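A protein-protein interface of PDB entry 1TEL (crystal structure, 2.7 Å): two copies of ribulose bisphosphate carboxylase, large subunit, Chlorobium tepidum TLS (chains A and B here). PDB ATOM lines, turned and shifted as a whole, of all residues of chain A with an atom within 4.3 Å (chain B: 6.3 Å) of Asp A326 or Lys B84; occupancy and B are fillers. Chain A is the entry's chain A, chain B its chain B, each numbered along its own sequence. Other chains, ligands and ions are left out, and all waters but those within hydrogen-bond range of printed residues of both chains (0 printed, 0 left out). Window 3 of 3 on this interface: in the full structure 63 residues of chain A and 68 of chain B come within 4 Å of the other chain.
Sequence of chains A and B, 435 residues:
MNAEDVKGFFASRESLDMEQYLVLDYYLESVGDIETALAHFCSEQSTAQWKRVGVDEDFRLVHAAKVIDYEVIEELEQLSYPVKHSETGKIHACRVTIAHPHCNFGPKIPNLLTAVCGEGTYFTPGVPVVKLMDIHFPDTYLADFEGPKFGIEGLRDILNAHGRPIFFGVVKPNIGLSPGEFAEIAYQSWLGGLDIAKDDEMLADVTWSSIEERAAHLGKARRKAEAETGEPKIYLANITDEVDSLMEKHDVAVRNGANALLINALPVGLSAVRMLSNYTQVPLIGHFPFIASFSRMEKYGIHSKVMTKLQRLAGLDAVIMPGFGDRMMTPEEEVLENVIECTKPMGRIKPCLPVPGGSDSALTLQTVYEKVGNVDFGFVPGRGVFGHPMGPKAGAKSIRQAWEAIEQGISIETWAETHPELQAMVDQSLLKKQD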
ATOM      1  N   PHE A 324      22.545  13.627  31.553  1.00  0.00           N
ATOM      2  CA  PHE A 324      21.559  14.471  32.198  1.00  0.00           C
ATOM      3  C   PHE A 324      22.065  15.818  32.643  1.00  0.00           C
ATOM      4  O   PHE A 324      21.374  16.516  33.377  1.00  0.00           O
ATOM      5  CB  PHE A 324      20.966  13.761  33.409  1.00  0.00           C
ATOM      6  CG  PHE A 324      20.073  12.638  33.051  1.00  0.00           C
ATOM      7  CD1 PHE A 324      18.946  12.860  32.267  1.00  0.00           C
ATOM      8  CD2 PHE A 324      20.355  11.347  33.477  1.00  0.00           C
ATOM      9  CE1 PHE A 324      18.110  11.812  31.908  1.00  0.00           C
ATOM     10  CE2 PHE A 324      19.522  10.284  33.126  1.00  0.00           C
ATOM     11  CZ  PHE A 324      18.396  10.519  32.338  1.00  0.00           C
ATOM     12  N   GLY A 325      23.268  16.187  32.236  1.00  0.00           N
ATOM     13  CA  GLY A 325      23.750  17.493  32.627  1.00  0.00           C
ATOM     14  C   GLY A 325      22.791  18.562  32.102  1.00  0.00           C
ATOM     15  O   GLY A 325      21.619  18.638  32.486  1.00  0.00           O
ATOM     16  N   ASP A 326      23.311  19.382  31.199  1.00  0.00           N
ATOM     17  CA  ASP A 326      22.595  20.476  30.548  1.00  0.00           C
ATOM     18  C   ASP A 326      23.756  21.255  30.002  1.00  0.00           C
ATOM     19  O   ASP A 326      23.607  22.259  29.310  1.00  0.00           O
ATOM     20  CB  ASP A 326      21.799  21.323  31.546  1.00  0.00           C
ATOM     21  CG  ASP A 326      20.352  20.863  31.675  1.00  0.00           C
ATOM     22  OD1 ASP A 326      19.737  20.519  30.634  1.00  0.00           O
ATOM     23  OD2 ASP A 326      19.828  20.859  32.814  1.00  0.00           O
ATOM     24  N   ARG A 327      24.926  20.730  30.338  1.00  0.00           N
ATOM     25  CA  ARG A 327      26.204  21.252  29.928  1.00  0.00           C
ATOM     26  C   ARG A 327      26.626  20.318  28.801  1.00  0.00           C
ATOM     27  O   ARG A 327      27.679  20.491  28.183  1.00  0.00           O
ATOM     28  CB  ARG A 327      27.159  21.177  31.114  1.00  0.00           C
ATOM     29  CG  ARG A 327      26.502  21.736  32.382  1.00  0.00           C
ATOM     30  CD  ARG A 327      27.377  21.624  33.620  1.00  0.00           C
ATOM     31  NE  ARG A 327      26.741  22.241  34.787  1.00  0.00           N
ATOM     32  CZ  ARG A 327      27.240  22.209  36.023  1.00  0.00           C
ATOM     33  NH1 ARG A 327      28.390  21.588  36.268  1.00  0.00           N
ATOM     34  NH2 ARG A 327      26.591  22.800  37.021  1.00  0.00           N
ATOM     35  N   MET A 328      25.778  19.321  28.549  1.00  0.00           N
ATOM     36  CA  MET A 328      26.005  18.363  27.486  1.00  0.00           C
ATOM     37  C   MET A 328      24.964  18.550  26.394  1.00  0.00           C
ATOM     38  O   MET A 328      24.724  17.664  25.591  1.00  0.00           O
ATOM     39  CB  MET A 328      25.974  16.938  28.024  1.00  0.00           C
ATOM     40  CG  MET A 328      27.233  16.559  28.794  1.00  0.00           C
ATOM     41  SD  MET A 328      28.761  17.091  27.950  1.00  0.00           S
ATOM     42  CE  MET A 328      28.934  15.820  26.681  1.00  0.00           C
ATOM     43  N   MET A 329      24.343  19.725  26.397  1.00  0.00           N
ATOM     44  CA  MET A 329      23.353  20.143  25.401  1.00  0.00           C
ATOM     45  C   MET A 329      22.329  19.134  24.895  1.00  0.00           C
ATOM     46  O   MET A 329      22.044  19.083  23.697  1.00  0.00           O
ATOM     47  CB  MET A 329      24.093  20.744  24.206  1.00  0.00           C
ATOM     48  CG  MET A 329      24.911  21.956  24.577  1.00  0.00           C
ATOM     49  SD  MET A 329      25.864  22.527  23.201  1.00  0.00           S
ATOM     50  CE  MET A 329      27.491  22.577  23.893  1.00  0.00           C
ATOM     51  N   PRO A 331      18.363  17.524  25.804  1.00  0.00           N
ATOM     52  CA  PRO A 331      17.198  17.579  26.682  1.00  0.00           C
ATOM     53  C   PRO A 331      17.113  16.275  27.475  1.00  0.00           C
ATOM     54  O   PRO A 331      17.355  15.198  26.931  1.00  0.00           O
ATOM     55  CB  PRO A 331      16.043  17.749  25.697  1.00  0.00           C
ATOM     56  CG  PRO A 331      16.680  18.449  24.526  1.00  0.00           C
ATOM     57  CD  PRO A 331      17.972  17.707  24.394  1.00  0.00           C
ATOM     58  N   GLU A 332      16.779  16.383  28.757  1.00  0.00           N
ATOM     59  CA  GLU A 332      16.672  15.217  29.622  1.00  0.00           C
ATOM     60  C   GLU A 332      15.859  14.105  28.949  1.00  0.00           C
ATOM     61  O   GLU A 332      16.230  12.927  29.017  1.00  0.00           O
ATOM     62  CB  GLU A 332      16.011  15.599  30.961  1.00  0.00           C
ATOM     63  CG  GLU A 332      16.556  16.874  31.626  1.00  0.00           C
ATOM     64  CD  GLU A 332      17.946  16.714  32.258  1.00  0.00           C
ATOM     65  OE1 GLU A 332      18.043  16.226  33.412  1.00  0.00           O
ATOM     66  OE2 GLU A 332      18.947  17.084  31.591  1.00  0.00           O
ATOM     67  N   SER A 359      28.701  15.911  32.903  1.00  0.00           N
ATOM     68  CA  SER A 359      28.874  16.974  33.875  1.00  0.00           C
ATOM     69  C   SER A 359      28.473  16.485  35.253  1.00  0.00           C
ATOM     70  O   SER A 359      27.807  17.183  36.023  1.00  0.00           O
ATOM     71  CB  SER A 359      28.037  18.205  33.469  1.00  0.00           C
ATOM     72  OG  SER A 359      26.668  17.887  33.253  1.00  0.00           O
ATOM     73  N   LEU B  79      21.214  32.478  18.596  1.00  0.00           N
ATOM     74  CA  LEU B  79      21.923  31.449  17.852  1.00  0.00           C
ATOM     75  C   LEU B  79      21.139  31.192  16.570  1.00  0.00           C
ATOM     76  O   LEU B  79      19.953  31.524  16.491  1.00  0.00           O
ATOM     77  CB  LEU B  79      21.992  30.160  18.666  1.00  0.00           C
ATOM     78  CG  LEU B  79      22.720  30.176  20.006  1.00  0.00           C
ATOM     79  CD1 LEU B  79      22.631  28.786  20.621  1.00  0.00           C
ATOM     80  CD2 LEU B  79      24.162  30.580  19.816  1.00  0.00           C
ATOM     81  N   TYR B  81      20.392  28.319  15.510  1.00  0.00           N
ATOM     82  CA  TYR B  81      19.574  27.137  15.789  1.00  0.00           C
ATOM     83  C   TYR B  81      19.323  27.071  17.297  1.00  0.00           C
ATOM     84  O   TYR B  81      20.256  27.206  18.090  1.00  0.00           O
ATOM     85  CB  TYR B  81      20.297  25.862  15.326  1.00  0.00           C
ATOM     86  CG  TYR B  81      20.789  25.925  13.897  1.00  0.00           C
ATOM     87  CD1 TYR B  81      22.153  25.996  13.608  1.00  0.00           C
ATOM     88  CD2 TYR B  81      19.884  25.955  12.834  1.00  0.00           C
ATOM     89  CE1 TYR B  81      22.601  26.103  12.294  1.00  0.00           C
ATOM     90  CE2 TYR B  81      20.317  26.061  11.514  1.00  0.00           C
ATOM     91  CZ  TYR B  81      21.671  26.140  11.252  1.00  0.00           C
ATOM     92  OH  TYR B  81      22.077  26.299   9.952  1.00  0.00           O
ATOM     93  N   PRO B  82      18.060  26.878  17.713  1.00  0.00           N
ATOM     94  CA  PRO B  82      17.667  26.796  19.129  1.00  0.00           C
ATOM     95  C   PRO B  82      18.266  25.603  19.882  1.00  0.00           C
ATOM     96  O   PRO B  82      17.586  24.611  20.133  1.00  0.00           O
ATOM     97  CB  PRO B  82      16.147  26.723  19.056  1.00  0.00           C
ATOM     98  CG  PRO B  82      15.916  26.002  17.752  1.00  0.00           C
ATOM     99  CD  PRO B  82      16.893  26.691  16.833  1.00  0.00           C
ATOM    100  N   VAL B  83      19.536  25.714  20.253  1.00  0.00           N
ATOM    101  CA  VAL B  83      20.241  24.653  20.956  1.00  0.00           C
ATOM    102  C   VAL B  83      20.258  24.881  22.466  1.00  0.00           C
ATOM    103  O   VAL B  83      20.575  25.974  22.935  1.00  0.00           O
ATOM    104  CB  VAL B  83      21.683  24.561  20.445  1.00  0.00           C
ATOM    105  CG1 VAL B  83      22.454  23.497  21.216  1.00  0.00           C
ATOM    106  CG2 VAL B  83      21.672  24.264  18.963  1.00  0.00           C
ATOM    107  N   LYS B  84      19.905  23.846  23.220  1.00  0.00           N
ATOM    108  CA  LYS B  84      19.873  23.901  24.679  1.00  0.00           C
ATOM    109  C   LYS B  84      21.281  23.891  25.258  1.00  0.00           C
ATOM    110  O   LYS B  84      21.966  22.865  25.228  1.00  0.00           O
ATOM    111  CB  LYS B  84      19.078  22.701  25.207  1.00  0.00           C
ATOM    112  CG  LYS B  84      19.231  22.382  26.699  1.00  0.00           C
ATOM    113  CD  LYS B  84      18.074  21.469  27.160  1.00  0.00           C
ATOM    114  CE  LYS B  84      16.695  22.158  26.959  1.00  0.00           C
ATOM    115  NZ  LYS B  84      15.491  21.257  27.020  1.00  0.00           N
ATOM    116  N   HIS B  85      21.718  25.035  25.776  1.00  0.00           N
ATOM    117  CA  HIS B  85      23.046  25.122  26.368  1.00  0.00           C
ATOM    118  C   HIS B  85      23.066  25.956  27.649  1.00  0.00           C
ATOM    119  O   HIS B  85      22.139  26.717  27.939  1.00  0.00           O
ATOM    120  CB  HIS B  85      24.049  25.672  25.353  1.00  0.00           C
ATOM    121  CG  HIS B  85      23.833  27.110  25.016  1.00  0.00           C
ATOM    122  ND1 HIS B  85      24.283  28.136  25.819  1.00  0.00           N
ATOM    123  CD2 HIS B  85      23.189  27.694  23.978  1.00  0.00           C
ATOM    124  CE1 HIS B  85      23.924  29.292  25.289  1.00  0.00           C
ATOM    125  NE2 HIS B  85      23.259  29.052  24.172  1.00  0.00           N
ATOM    126  N   SER B  86      24.145  25.789  28.404  1.00  0.00           N
ATOM    127  CA  SER B  86      24.348  26.450  29.691  1.00  0.00           C
ATOM    128  C   SER B  86      24.745  27.917  29.651  1.00  0.00           C
ATOM    129  O   SER B  86      24.152  28.749  30.340  1.00  0.00           O
ATOM    130  CB  SER B  86      25.404  25.672  30.488  1.00  0.00           C
ATOM    131  OG  SER B  86      26.515  25.306  29.674  1.00  0.00           O
ATOM    132  N   PRO B 128      27.959  26.360  21.136  1.00  0.00           N
ATOM    133  CA  PRO B 128      26.845  25.467  20.801  1.00  0.00           C
ATOM    134  C   PRO B 128      26.520  25.220  19.326  1.00  0.00           C
ATOM    135  O   PRO B 128      25.798  24.281  19.006  1.00  0.00           O
ATOM    136  CB  PRO B 128      25.681  26.105  21.551  1.00  0.00           C
ATOM    137  CG  PRO B 128      25.963  27.561  21.359  1.00  0.00           C
ATOM    138  CD  PRO B 128      27.461  27.672  21.586  1.00  0.00           C
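Among the printed residues, merely in contact across the chains: Asp A326 with Lys B84 (3.97 Å), Asp A326 with Ser B86 (3.7 Å), Met A329 with Lys B84 (3.1 Å), Met A329 with His B85 (3.9 Å), Met A329 with Pro B128 (3.9 Å) and Pro A331 with Lys B84 (3.8 Å).
Of chain B, only Lys B84 (3.97 Å) and Ser B86 (3.7 Å) come within 4 Å of Asp A326. Printed residues of chain B within 4 Å of Met A329: Lys B84, His B85 and Pro B128. Of the printed residues of chain B, Pro A331 touches Lys B84 (3.8 Å). Of chain A, only Asp A326 (3.97 Å), Met A329 (3.1 Å) and Pro A331 (3.8 Å) come within 4 Å of Lys B84. Of the printed residues of chain A, His B85 touches Met A329. Of the printed residues of chain A, Ser B86 touches Asp A326. Printed residues of chain A within 4 Å of Pro B128: Met A329 (3.9 Å). The nearest printed residue of chain A that does not touch Lys B84 is Glu A332 (5.3 Å).
Printed residues of chain A that touch a printed residue of chain B: Asp A326, Met A329 and Pro A331. Hydrophobic or aromatic side chains of chain A within 4 Å of the printed part of chain B: Met A329 and Pro A331. Along chain A the printed residues that touch a printed residue of chain B span positions 326 to 331. Of the 8 printed residues of chain B, 4 touch a printed residue of chain A. Hydrophobic or aromatic side chains of chain B within 4 Å of the printed part of chain A: His B85 and Pro B128. Among the printed residues, no Asp or Glu carboxylate lies within 4 Å of a Lys or Arg side-chain nitrogen of the other chain.
No position is printed for both chains. Of the 6 pairs that touch across the chains among the printed residues, none has its exchanged pair printed and touching as well.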
